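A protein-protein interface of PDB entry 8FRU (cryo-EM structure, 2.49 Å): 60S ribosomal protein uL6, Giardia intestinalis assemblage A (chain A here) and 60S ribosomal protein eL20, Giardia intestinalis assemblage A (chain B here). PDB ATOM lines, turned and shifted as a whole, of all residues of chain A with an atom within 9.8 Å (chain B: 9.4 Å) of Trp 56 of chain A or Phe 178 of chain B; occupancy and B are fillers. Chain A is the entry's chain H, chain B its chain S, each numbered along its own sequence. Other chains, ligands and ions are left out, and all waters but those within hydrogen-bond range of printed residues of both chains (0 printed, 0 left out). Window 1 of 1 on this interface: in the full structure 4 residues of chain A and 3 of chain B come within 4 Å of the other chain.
NH2 of Arg 62 of chain A is in hydrogen-bond range of O of Trp 56 of chain A, at 3.4 Å. The guanidinium group (NH2) of Arg 62 of chain A lies within hydrogen-bond range of the backbone carbonyl oxygen (O) of Phe 57 of chain A. The backbone NH (N) of Phe 57 of chain A sits at hydrogen-bond distance from the backbone carbonyl oxygen (O) of Leu 3 of chain A.
Among the printed residues, merely in contact across the chains: Pro 2 of chain A with Met 170 of chain B, Phe 57 of chain A with Pro 179 of chain B, Trp 56 of chain A with Pro 179 of chain B, Leu 3 of chain A with Met 170 of chain B and Trp 56 of chain A with Phe 178 of chain B.
Of the printed residues of chain B, Trp 56 of chain A touches Phe 178 and Pro 179. No residue of chain B comes within 4 Å of Val 55 of chain A. Of the printed residues of chain A, Met 170 of chain B touches Pro 2 (3.3 Å) and Leu 3 (3.97 Å). Of the printed residues of chain B, Pro 2 of chain A touches Met 170. Of the printed residues of chain B, Leu 3 of chain A touches Met 170 (3.97 Å). The nearest printed residue of chain B that does not touch Trp 56 of chain A is Arg 177 of chain B (4.01 Å). The nearest residue of chain A that does not touch Phe 178 of chain B is Leu 3 of chain A (4.1 Å).
Hydrophobic or aromatic side chains of chain B within 4 Å of the printed part of chain A: Met 170, Phe 178 and Pro 179. Of the 25 printed residues of chain A, 4 touch a printed residue of chain B. Among the printed residues, 5 pairs touch across the chains.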
ATOM      1  N   MET A   1       2.243 -22.310 -32.001  1.00  0.00           N
ATOM      2  CA  MET A   1       1.982 -21.652 -30.728  1.00  0.00           C
ATOM      3  C   MET A   1       3.294 -21.209 -30.079  1.00  0.00           C
ATOM      4  O   MET A   1       4.353 -21.758 -30.377  1.00  0.00           O
ATOM      5  CB  MET A   1       1.184 -22.579 -29.797  1.00  0.00           C
ATOM      6  CG  MET A   1       1.516 -22.463 -28.317  1.00  0.00           C
ATOM      7  SD  MET A   1       0.931 -23.870 -27.351  1.00  0.00           S
ATOM      8  CE  MET A   1       2.118 -23.893 -26.012  1.00  0.00           C
ATOM      9  N   PRO A   2       3.223 -20.202 -29.205  1.00  0.00           N
ATOM     10  CA  PRO A   2       4.459 -19.651 -28.630  1.00  0.00           C
ATOM     11  C   PRO A   2       5.329 -20.676 -27.921  1.00  0.00           C
ATOM     12  O   PRO A   2       6.554 -20.650 -28.083  1.00  0.00           O
ATOM     13  CB  PRO A   2       3.933 -18.590 -27.657  1.00  0.00           C
ATOM     14  CG  PRO A   2       2.641 -18.156 -28.259  1.00  0.00           C
ATOM     15  CD  PRO A   2       2.038 -19.411 -28.832  1.00  0.00           C
ATOM     16  N   LEU A   3       4.740 -21.583 -27.145  1.00  0.00           N
ATOM     17  CA  LEU A   3       5.550 -22.531 -26.390  1.00  0.00           C
ATOM     18  C   LEU A   3       5.758 -23.839 -27.141  1.00  0.00           C
ATOM     19  O   LEU A   3       6.858 -24.399 -27.109  1.00  0.00           O
ATOM     20  CB  LEU A   3       4.915 -22.800 -25.024  1.00  0.00           C
ATOM     21  CG  LEU A   3       5.889 -22.967 -23.858  1.00  0.00           C
ATOM     22  CD1 LEU A   3       7.187 -22.247 -24.145  1.00  0.00           C
ATOM     23  CD2 LEU A   3       5.281 -22.448 -22.575  1.00  0.00           C
ATOM     24  N   CYS A   4       4.726 -24.339 -27.813  1.00  0.00           N
ATOM     25  CA  CYS A   4       4.856 -25.500 -28.679  1.00  0.00           C
ATOM     26  C   CYS A   4       3.771 -25.443 -29.740  1.00  0.00           C
ATOM     27  O   CYS A   4       2.631 -25.078 -29.451  1.00  0.00           O
ATOM     28  CB  CYS A   4       4.748 -26.814 -27.898  1.00  0.00           C
ATOM     29  SG  CYS A   4       3.071 -27.266 -27.433  1.00  0.00           S
ATOM     30  N   SER A   5       4.132 -25.804 -30.965  1.00  0.00           N
ATOM     31  CA  SER A   5       3.188 -25.903 -32.067  1.00  0.00           C
ATOM     32  C   SER A   5       2.823 -27.364 -32.275  1.00  0.00           C
ATOM     33  O   SER A   5       3.706 -28.220 -32.376  1.00  0.00           O
ATOM     34  CB  SER A   5       3.777 -25.319 -33.349  1.00  0.00           C
ATOM     35  OG  SER A   5       4.043 -23.940 -33.193  1.00  0.00           O
ATOM     36  N   SER A   6       1.525 -27.648 -32.321  1.00  0.00           N
ATOM     37  CA  SER A   6       1.041 -29.009 -32.462  1.00  0.00           C
ATOM     38  C   SER A   6      -0.170 -29.030 -33.380  1.00  0.00           C
ATOM     39  O   SER A   6      -0.883 -28.034 -33.515  1.00  0.00           O
ATOM     40  CB  SER A   6       0.676 -29.620 -31.105  1.00  0.00           C
ATOM     41  OG  SER A   6      -0.362 -30.576 -31.238  1.00  0.00           O
ATOM     42  N   PRO A  41      12.914 -33.169 -35.746  1.00  0.00           N
ATOM     43  CA  PRO A  41      12.641 -33.319 -34.310  1.00  0.00           C
ATOM     44  C   PRO A  41      11.164 -33.182 -33.976  1.00  0.00           C
ATOM     45  O   PRO A  41      10.631 -32.071 -33.984  1.00  0.00           O
ATOM     46  CB  PRO A  41      13.461 -32.187 -33.685  1.00  0.00           C
ATOM     47  CG  PRO A  41      13.512 -31.142 -34.742  1.00  0.00           C
ATOM     48  CD  PRO A  41      13.407 -31.822 -36.081  1.00  0.00           C
ATOM     49  N   LEU A  42      10.495 -34.292 -33.674  1.00  0.00           N
ATOM     50  CA  LEU A  42       9.048 -34.297 -33.525  1.00  0.00           C
ATOM     51  C   LEU A  42       8.641 -35.145 -32.332  1.00  0.00           C
ATOM     52  O   LEU A  42       9.349 -36.066 -31.922  1.00  0.00           O
ATOM     53  CB  LEU A  42       8.356 -34.844 -34.773  1.00  0.00           C
ATOM     54  CG  LEU A  42       8.759 -34.274 -36.124  1.00  0.00           C
ATOM     55  CD1 LEU A  42       8.794 -35.395 -37.136  1.00  0.00           C
ATOM     56  CD2 LEU A  42       7.801 -33.190 -36.563  1.00  0.00           C
ATOM     57  N   ASP A  43       7.467 -34.835 -31.794  1.00  0.00           N
ATOM     58  CA  ASP A  43       6.832 -35.622 -30.743  1.00  0.00           C
ATOM     59  C   ASP A  43       5.506 -36.143 -31.280  1.00  0.00           C
ATOM     60  O   ASP A  43       4.543 -35.381 -31.404  1.00  0.00           O
ATOM     61  CB  ASP A  43       6.629 -34.786 -29.483  1.00  0.00           C
ATOM     62  CG  ASP A  43       6.407 -35.633 -28.251  1.00  0.00           C
ATOM     63  OD1 ASP A  43       6.539 -36.871 -28.350  1.00  0.00           O
ATOM     64  OD2 ASP A  43       6.103 -35.063 -27.183  1.00  0.00           O
ATOM     65  N   ILE A  44       5.456 -37.433 -31.601  1.00  0.00           N
ATOM     66  CA  ILE A  44       4.263 -38.077 -32.137  1.00  0.00           C
ATOM     67  C   ILE A  44       3.638 -38.930 -31.046  1.00  0.00           C
ATOM     68  O   ILE A  44       4.317 -39.762 -30.436  1.00  0.00           O
ATOM     69  CB  ILE A  44       4.582 -38.931 -33.374  1.00  0.00           C
ATOM     70  CG1 ILE A  44       4.994 -38.048 -34.546  1.00  0.00           C
ATOM     71  CG2 ILE A  44       3.382 -39.778 -33.749  1.00  0.00           C
ATOM     72  CD1 ILE A  44       6.458 -38.132 -34.884  1.00  0.00           C
ATOM     73  N   THR A  45       2.344 -38.734 -30.810  1.00  0.00           N
ATOM     74  CA  THR A  45       1.619 -39.453 -29.775  1.00  0.00           C
ATOM     75  C   THR A  45       0.321 -40.012 -30.339  1.00  0.00           C
ATOM     76  O   THR A  45      -0.320 -39.398 -31.193  1.00  0.00           O
ATOM     77  CB  THR A  45       1.306 -38.551 -28.583  1.00  0.00           C
ATOM     78  OG1 THR A  45       2.392 -37.640 -28.376  1.00  0.00           O
ATOM     79  CG2 THR A  45       1.097 -39.383 -27.330  1.00  0.00           C
ATOM     80  N   SER A  52      -1.299 -36.956 -32.984  1.00  0.00           N
ATOM     81  CA  SER A  52      -0.947 -35.569 -32.725  1.00  0.00           C
ATOM     82  C   SER A  52       0.559 -35.392 -32.853  1.00  0.00           C
ATOM     83  O   SER A  52       1.332 -36.225 -32.375  1.00  0.00           O
ATOM     84  CB  SER A  52      -1.415 -35.132 -31.338  1.00  0.00           C
ATOM     85  OG  SER A  52      -0.574 -35.659 -30.330  1.00  0.00           O
ATOM     86  N   VAL A  53       0.970 -34.305 -33.500  1.00  0.00           N
ATOM     87  CA  VAL A  53       2.376 -34.002 -33.735  1.00  0.00           C
ATOM     88  C   VAL A  53       2.682 -32.645 -33.121  1.00  0.00           C
ATOM     89  O   VAL A  53       2.010 -31.655 -33.429  1.00  0.00           O
ATOM     90  CB  VAL A  53       2.713 -34.006 -35.236  1.00  0.00           C
ATOM     91  CG1 VAL A  53       4.188 -33.730 -35.451  1.00  0.00           C
ATOM     92  CG2 VAL A  53       2.318 -35.325 -35.861  1.00  0.00           C
ATOM     93  N   ALA A  54       3.697 -32.595 -32.264  1.00  0.00           N
ATOM     94  CA  ALA A  54       4.054 -31.374 -31.558  1.00  0.00           C
ATOM     95  C   ALA A  54       5.544 -31.106 -31.694  1.00  0.00           C
ATOM     96  O   ALA A  54       6.352 -32.035 -31.716  1.00  0.00           O
ATOM     97  CB  ALA A  54       3.675 -31.461 -30.080  1.00  0.00           C
ATOM     98  N   VAL A  55       5.898 -29.828 -31.787  1.00  0.00           N
ATOM     99  CA  VAL A  55       7.285 -29.381 -31.797  1.00  0.00           C
ATOM    100  C   VAL A  55       7.445 -28.339 -30.702  1.00  0.00           C
ATOM    101  O   VAL A  55       6.716 -27.344 -30.678  1.00  0.00           O
ATOM    102  CB  VAL A  55       7.695 -28.799 -33.164  1.00  0.00           C
ATOM    103  CG1 VAL A  55       8.974 -28.012 -33.042  1.00  0.00           C
ATOM    104  CG2 VAL A  55       7.861 -29.906 -34.185  1.00  0.00           C
ATOM    105  N   TRP A  56       8.391 -28.563 -29.803  1.00  0.00           N
ATOM    106  CA  TRP A  56       8.607 -27.663 -28.682  1.00  0.00           C
ATOM    107  C   TRP A  56       9.572 -26.554 -29.066  1.00  0.00           C
ATOM    108  O   TRP A  56      10.553 -26.786 -29.774  1.00  0.00           O
ATOM    109  CB  TRP A  56       9.146 -28.429 -27.478  1.00  0.00           C
ATOM    110  CG  TRP A  56       8.123 -29.261 -26.795  1.00  0.00           C
ATOM    111  CD1 TRP A  56       7.932 -30.598 -26.934  1.00  0.00           C
ATOM    112  CD2 TRP A  56       7.148 -28.811 -25.855  1.00  0.00           C
ATOM    113  NE1 TRP A  56       6.900 -31.014 -26.137  1.00  0.00           N
ATOM    114  CE2 TRP A  56       6.400 -29.933 -25.464  1.00  0.00           C
ATOM    115  CE3 TRP A  56       6.837 -27.570 -25.303  1.00  0.00           C
ATOM    116  CZ2 TRP A  56       5.361 -29.850 -24.553  1.00  0.00           C
ATOM    117  CZ3 TRP A  56       5.807 -27.491 -24.396  1.00  0.00           C
ATOM    118  CH2 TRP A  56       5.081 -28.621 -24.030  1.00  0.00           C
ATOM    119  N   PHE A  57       9.288 -25.347 -28.593  1.00  0.00           N
ATOM    120  CA  PHE A  57      10.121 -24.185 -28.868  1.00  0.00           C
ATOM    121  C   PHE A  57      10.174 -23.903 -30.363  1.00  0.00           C
ATOM    122  O   PHE A  57      11.249 -23.982 -30.970  1.00  0.00           O
ATOM    123  CB  PHE A  57      11.533 -24.395 -28.326  1.00  0.00           C
ATOM    124  CG  PHE A  57      11.571 -24.871 -26.906  1.00  0.00           C
ATOM    125  CD1 PHE A  57      11.064 -24.089 -25.889  1.00  0.00           C
ATOM    126  CD2 PHE A  57      12.110 -26.101 -26.591  1.00  0.00           C
ATOM    127  CE1 PHE A  57      11.094 -24.523 -24.587  1.00  0.00           C
ATOM    128  CE2 PHE A  57      12.143 -26.539 -25.291  1.00  0.00           C
ATOM    129  CZ  PHE A  57      11.634 -25.748 -24.286  1.00  0.00           C
ATOM    130  N   PRO A  58       9.057 -23.552 -30.984  1.00  0.00           N
ATOM    131  CA  PRO A  58       9.045 -23.385 -32.442  1.00  0.00           C
ATOM    132  C   PRO A  58       9.753 -22.117 -32.878  1.00  0.00           C
ATOM    133  O   PRO A  58       9.153 -21.040 -32.869  1.00  0.00           O
ATOM    134  CB  PRO A  58       7.549 -23.322 -32.778  1.00  0.00           C
ATOM    135  CG  PRO A  58       6.819 -23.504 -31.472  1.00  0.00           C
ATOM    136  CD  PRO A  58       7.771 -23.181 -30.387  1.00  0.00           C
ATOM    137  N   ARG A  59      11.017 -22.223 -33.269  1.00  0.00           N
ATOM    138  CA  ARG A  59      11.836 -21.065 -33.603  1.00  0.00           C
ATOM    139  C   ARG A  59      12.246 -21.149 -35.065  1.00  0.00           C
ATOM    140  O   ARG A  59      12.868 -22.131 -35.483  1.00  0.00           O
ATOM    141  CB  ARG A  59      13.062 -21.000 -32.691  1.00  0.00           C
ATOM    142  CG  ARG A  59      14.144 -20.038 -33.132  1.00  0.00           C
ATOM    143  CD  ARG A  59      13.783 -18.608 -32.789  1.00  0.00           C
ATOM    144  NE  ARG A  59      14.916 -17.704 -32.946  1.00  0.00           N
ATOM    145  CZ  ARG A  59      15.585 -17.158 -31.940  1.00  0.00           C
ATOM    146  NH1 ARG A  59      15.270 -17.415 -30.681  1.00  0.00           N
ATOM    147  NH2 ARG A  59      16.588 -16.326 -32.202  1.00  0.00           N
ATOM    148  N   GLY A  60      11.898 -20.127 -35.835  1.00  0.00           N
ATOM    149  CA  GLY A  60      12.318 -20.074 -37.227  1.00  0.00           C
ATOM    150  C   GLY A  60      11.496 -20.994 -38.097  1.00  0.00           C
ATOM    151  O   GLY A  60      10.266 -20.930 -38.101  1.00  0.00           O
ATOM    152  N   LYS A  61      12.178 -21.864 -38.840  1.00  0.00           N
ATOM    153  CA  LYS A  61      11.523 -22.779 -39.766  1.00  0.00           C
ATOM    154  C   LYS A  61      11.031 -24.059 -39.103  1.00  0.00           C
ATOM    155  O   LYS A  61      10.474 -24.914 -39.793  1.00  0.00           O
ATOM    156  CB  LYS A  61      12.469 -23.131 -40.916  1.00  0.00           C
ATOM    157  CG  LYS A  61      12.537 -22.082 -42.015  1.00  0.00           C
ATOM    158  CD  LYS A  61      11.294 -22.098 -42.890  1.00  0.00           C
ATOM    159  CE  LYS A  61      11.204 -20.855 -43.764  1.00  0.00           C
ATOM    160  NZ  LYS A  61      12.508 -20.479 -44.372  1.00  0.00           N
ATOM    161  N   ARG A  62      11.230 -24.223 -37.795  1.00  0.00           N
ATOM    162  CA  ARG A  62      10.654 -25.365 -37.099  1.00  0.00           C
ATOM    163  C   ARG A  62       9.138 -25.307 -37.060  1.00  0.00           C
ATOM    164  O   ARG A  62       8.497 -26.326 -36.793  1.00  0.00           O
ATOM    165  CB  ARG A  62      11.185 -25.447 -35.672  1.00  0.00           C
ATOM    166  CG  ARG A  62      12.679 -25.464 -35.578  1.00  0.00           C
ATOM    167  CD  ARG A  62      13.150 -26.598 -34.700  1.00  0.00           C
ATOM    168  NE  ARG A  62      12.990 -26.320 -33.281  1.00  0.00           N
ATOM    169  CZ  ARG A  62      13.869 -26.674 -32.356  1.00  0.00           C
ATOM    170  NH1 ARG A  62      14.986 -27.306 -32.672  1.00  0.00           N
ATOM    171  NH2 ARG A  62      13.620 -26.391 -31.081  1.00  0.00           N
ATOM    172  N   ASN A  63       8.552 -24.142 -37.316  1.00  0.00           N
ATOM    173  CA  ASN A  63       7.110 -23.973 -37.241  1.00  0.00           C
ATOM    174  C   ASN A  63       6.378 -24.561 -38.435  1.00  0.00           C
ATOM    175  O   ASN A  63       5.144 -24.590 -38.426  1.00  0.00           O
ATOM    176  CB  ASN A  63       6.772 -22.489 -37.116  1.00  0.00           C
ATOM    177  CG  ASN A  63       5.461 -22.251 -36.412  1.00  0.00           C
ATOM    178  OD1 ASN A  63       5.248 -22.715 -35.296  1.00  0.00           O
ATOM    179  ND2 ASN A  63       4.569 -21.521 -37.063  1.00  0.00           N
ATOM    180  N   LEU A  65       6.848 -27.763 -39.669  1.00  0.00           N
ATOM    181  CA  LEU A  65       6.995 -29.215 -39.739  1.00  0.00           C
ATOM    182  C   LEU A  65       5.734 -29.990 -39.361  1.00  0.00           C
ATOM    183  O   LEU A  65       5.398 -30.977 -40.031  1.00  0.00           O
ATOM    184  CB  LEU A  65       8.155 -29.665 -38.848  1.00  0.00           C
ATOM    185  CG  LEU A  65       9.554 -29.230 -39.283  1.00  0.00           C
ATOM    186  CD1 LEU A  65      10.572 -29.491 -38.191  1.00  0.00           C
ATOM    187  CD2 LEU A  65       9.956 -29.944 -40.564  1.00  0.00           C
ATOM    188  N   PRO A  66       5.033 -29.618 -38.287  1.00  0.00           N
ATOM    189  CA  PRO A  66       3.881 -30.437 -37.872  1.00  0.00           C
ATOM    190  C   PRO A  66       2.820 -30.597 -38.947  1.00  0.00           C
ATOM    191  O   PRO A  66       2.308 -31.706 -39.144  1.00  0.00           O
ATOM    192  CB  PRO A  66       3.350 -29.690 -36.637  1.00  0.00           C
ATOM    193  CG  PRO A  66       3.969 -28.343 -36.684  1.00  0.00           C
ATOM    194  CD  PRO A  66       5.285 -28.515 -37.349  1.00  0.00           C
ATOM    195  N   LYS B 167       5.785 -13.292 -25.095  1.00  0.00           N
ATOM    196  CA  LYS B 167       6.561 -14.181 -24.237  1.00  0.00           C
ATOM    197  C   LYS B 167       6.159 -14.024 -22.773  1.00  0.00           C
ATOM    198  O   LYS B 167       5.844 -15.010 -22.087  1.00  0.00           O
ATOM    199  CB  LYS B 167       8.048 -13.909 -24.430  1.00  0.00           C
ATOM    200  CG  LYS B 167       8.631 -14.620 -25.632  1.00  0.00           C
ATOM    201  CD  LYS B 167       9.516 -13.698 -26.451  1.00  0.00           C
ATOM    202  CE  LYS B 167      10.988 -13.971 -26.199  1.00  0.00           C
ATOM    203  NZ  LYS B 167      11.852 -12.930 -26.818  1.00  0.00           N
ATOM    204  N   MET B 170       2.637 -15.483 -22.260  1.00  0.00           N
ATOM    205  CA  MET B 170       2.605 -16.935 -22.191  1.00  0.00           C
ATOM    206  C   MET B 170       3.258 -17.465 -20.928  1.00  0.00           C
ATOM    207  O   MET B 170       3.002 -18.610 -20.548  1.00  0.00           O
ATOM    208  CB  MET B 170       3.273 -17.535 -23.425  1.00  0.00           C
ATOM    209  CG  MET B 170       4.781 -17.477 -23.423  1.00  0.00           C
ATOM    210  SD  MET B 170       5.469 -18.547 -24.697  1.00  0.00           S
ATOM    211  CE  MET B 170       7.022 -17.730 -25.039  1.00  0.00           C
ATOM    212  N   PHE B 171       4.098 -16.675 -20.270  1.00  0.00           N
ATOM    213  CA  PHE B 171       4.636 -17.136 -18.997  1.00  0.00           C
ATOM    214  C   PHE B 171       3.839 -16.667 -17.788  1.00  0.00           C
ATOM    215  O   PHE B 171       4.146 -17.090 -16.669  1.00  0.00           O
ATOM    216  CB  PHE B 171       6.095 -16.711 -18.858  1.00  0.00           C
ATOM    217  CG  PHE B 171       7.035 -17.609 -19.586  1.00  0.00           C
ATOM    218  CD1 PHE B 171       7.186 -18.921 -19.198  1.00  0.00           C
ATOM    219  CD2 PHE B 171       7.729 -17.157 -20.688  1.00  0.00           C
ATOM    220  CE1 PHE B 171       8.033 -19.755 -19.876  1.00  0.00           C
ATOM    221  CE2 PHE B 171       8.576 -17.991 -21.367  1.00  0.00           C
ATOM    222  CZ  PHE B 171       8.727 -19.291 -20.961  1.00  0.00           C
ATOM    223  N   GLY B 175      -0.330 -23.155 -14.391  1.00  0.00           N
ATOM    224  CA  GLY B 175      -0.043 -24.533 -14.758  1.00  0.00           C
ATOM    225  C   GLY B 175       0.763 -24.671 -16.029  1.00  0.00           C
ATOM    226  O   GLY B 175       0.514 -25.586 -16.821  1.00  0.00           O
ATOM    227  N   VAL B 176       1.736 -23.791 -16.234  1.00  0.00           N
ATOM    228  CA  VAL B 176       2.561 -23.818 -17.435  1.00  0.00           C
ATOM    229  C   VAL B 176       3.675 -24.842 -17.260  1.00  0.00           C
ATOM    230  O   VAL B 176       4.312 -24.916 -16.203  1.00  0.00           O
ATOM    231  CB  VAL B 176       3.117 -22.414 -17.731  1.00  0.00           C
ATOM    232  CG1 VAL B 176       3.489 -21.711 -16.444  1.00  0.00           C
ATOM    233  CG2 VAL B 176       4.306 -22.493 -18.665  1.00  0.00           C
ATOM    234  N   ARG B 177       3.901 -25.650 -18.296  1.00  0.00           N
ATOM    235  CA  ARG B 177       4.868 -26.736 -18.256  1.00  0.00           C
ATOM    236  C   ARG B 177       5.657 -26.769 -19.552  1.00  0.00           C
ATOM    237  O   ARG B 177       5.161 -26.368 -20.605  1.00  0.00           O
ATOM    238  CB  ARG B 177       4.191 -28.098 -18.068  1.00  0.00           C
ATOM    239  CG  ARG B 177       3.535 -28.304 -16.734  1.00  0.00           C
ATOM    240  CD  ARG B 177       2.421 -29.335 -16.834  1.00  0.00           C
ATOM    241  NE  ARG B 177       2.927 -30.700 -16.746  1.00  0.00           N
ATOM    242  CZ  ARG B 177       3.003 -31.539 -17.769  1.00  0.00           C
ATOM    243  NH1 ARG B 177       2.590 -31.195 -18.977  1.00  0.00           N
ATOM    244  NH2 ARG B 177       3.506 -32.754 -17.574  1.00  0.00           N
ATOM    245  N   PHE B 178       6.886 -27.258 -19.471  1.00  0.00           N
ATOM    246  CA  PHE B 178       7.675 -27.559 -20.657  1.00  0.00           C
ATOM    247  C   PHE B 178       8.885 -28.379 -20.233  1.00  0.00           C
ATOM    248  O   PHE B 178       9.275 -28.350 -19.068  1.00  0.00           O
ATOM    249  CB  PHE B 178       8.109 -26.282 -21.397  1.00  0.00           C
ATOM    250  CG  PHE B 178       8.725 -25.231 -20.519  1.00  0.00           C
ATOM    251  CD1 PHE B 178      10.086 -25.218 -20.285  1.00  0.00           C
ATOM    252  CD2 PHE B 178       7.949 -24.235 -19.962  1.00  0.00           C
ATOM    253  CE1 PHE B 178      10.654 -24.250 -19.499  1.00  0.00           C
ATOM    254  CE2 PHE B 178       8.515 -23.266 -19.169  1.00  0.00           C
ATOM    255  CZ  PHE B 178       9.867 -23.272 -18.940  1.00  0.00           C
ATOM    256  N   PRO B 179       9.466 -29.134 -21.156  1.00  0.00           N
ATOM    257  CA  PRO B 179      10.666 -29.912 -20.843  1.00  0.00           C
ATOM    258  C   PRO B 179      11.905 -29.029 -20.764  1.00  0.00           C
ATOM    259  O   PRO B 179      11.916 -27.878 -21.193  1.00  0.00           O
ATOM    260  CB  PRO B 179      10.756 -30.898 -22.012  1.00  0.00           C
ATOM    261  CG  PRO B 179       9.992 -30.272 -23.106  1.00  0.00           C
ATOM    262  CD  PRO B 179       8.924 -29.450 -22.485  1.00  0.00           C
ATOM    263  N   HIS B 180      12.965 -29.602 -20.206  1.00  0.00           N
ATOM    264  CA  HIS B 180      14.203 -28.859 -20.012  1.00  0.00           C
ATOM    265  C   HIS B 180      14.730 -28.359 -21.354  1.00  0.00           C
ATOM    266  O   HIS B 180      14.884 -29.152 -22.289  1.00  0.00           O
ATOM    267  CB  HIS B 180      15.248 -29.735 -19.328  1.00  0.00           C
ATOM    268  CG  HIS B 180      16.363 -28.963 -18.695  1.00  0.00           C
ATOM    269  ND1 HIS B 180      17.134 -28.063 -19.394  1.00  0.00           N
ATOM    270  CD2 HIS B 180      16.833 -28.953 -17.427  1.00  0.00           C
ATOM    271  CE1 HIS B 180      18.032 -27.534 -18.585  1.00  0.00           C
ATOM    272  NE2 HIS B 180      17.870 -28.058 -17.386  1.00  0.00           N
ATOM    273  N   PRO B 181      15.015 -27.062 -21.489  1.00  0.00           N
ATOM    274  CA  PRO B 181      15.363 -26.520 -22.812  1.00  0.00           C
ATOM    275  C   PRO B 181      16.753 -26.894 -23.305  1.00  0.00           C
ATOM    276  O   PRO B 181      17.002 -26.782 -24.509  1.00  0.00           O
ATOM    277  CB  PRO B 181      15.243 -25.002 -22.620  1.00  0.00           C
ATOM    278  CG  PRO B 181      14.605 -24.798 -21.301  1.00  0.00           C
ATOM    279  CD  PRO B 181      14.828 -26.011 -20.481  1.00  0.00           C
ATOM    280  N   CYS B 182      17.666 -27.325 -22.437  1.00  0.00           N
ATOM    281  CA  CYS B 182      19.046 -27.603 -22.837  1.00  0.00           C
ATOM    282  C   CYS B 182      19.670 -28.598 -21.870  1.00  0.00           C
ATOM    283  O   CYS B 182      20.597 -28.272 -21.124  1.00  0.00           O
ATOM    284  CB  CYS B 182      19.861 -26.313 -22.890  1.00  0.00           C
ATOM    285  SG  CYS B 182      19.686 -25.256 -21.439  1.00  0.00           S
ATOM    286  N   GLN B 205      15.882 -37.099 -19.866  1.00  0.00           N
ATOM    287  CA  GLN B 205      14.848 -36.116 -20.160  1.00  0.00           C
ATOM    288  C   GLN B 205      13.518 -36.504 -19.527  1.00  0.00           C
ATOM    289  O   GLN B 205      13.175 -37.682 -19.453  1.00  0.00           O
ATOM    290  CB  GLN B 205      14.677 -35.954 -21.671  1.00  0.00           C
ATOM    291  CG  GLN B 205      15.971 -35.802 -22.427  1.00  0.00           C
ATOM    292  CD  GLN B 205      15.876 -34.791 -23.545  1.00  0.00           C
ATOM    293  OE1 GLN B 205      15.285 -33.727 -23.387  1.00  0.00           O
ATOM    294  NE2 GLN B 205      16.459 -35.122 -24.688  1.00  0.00           N
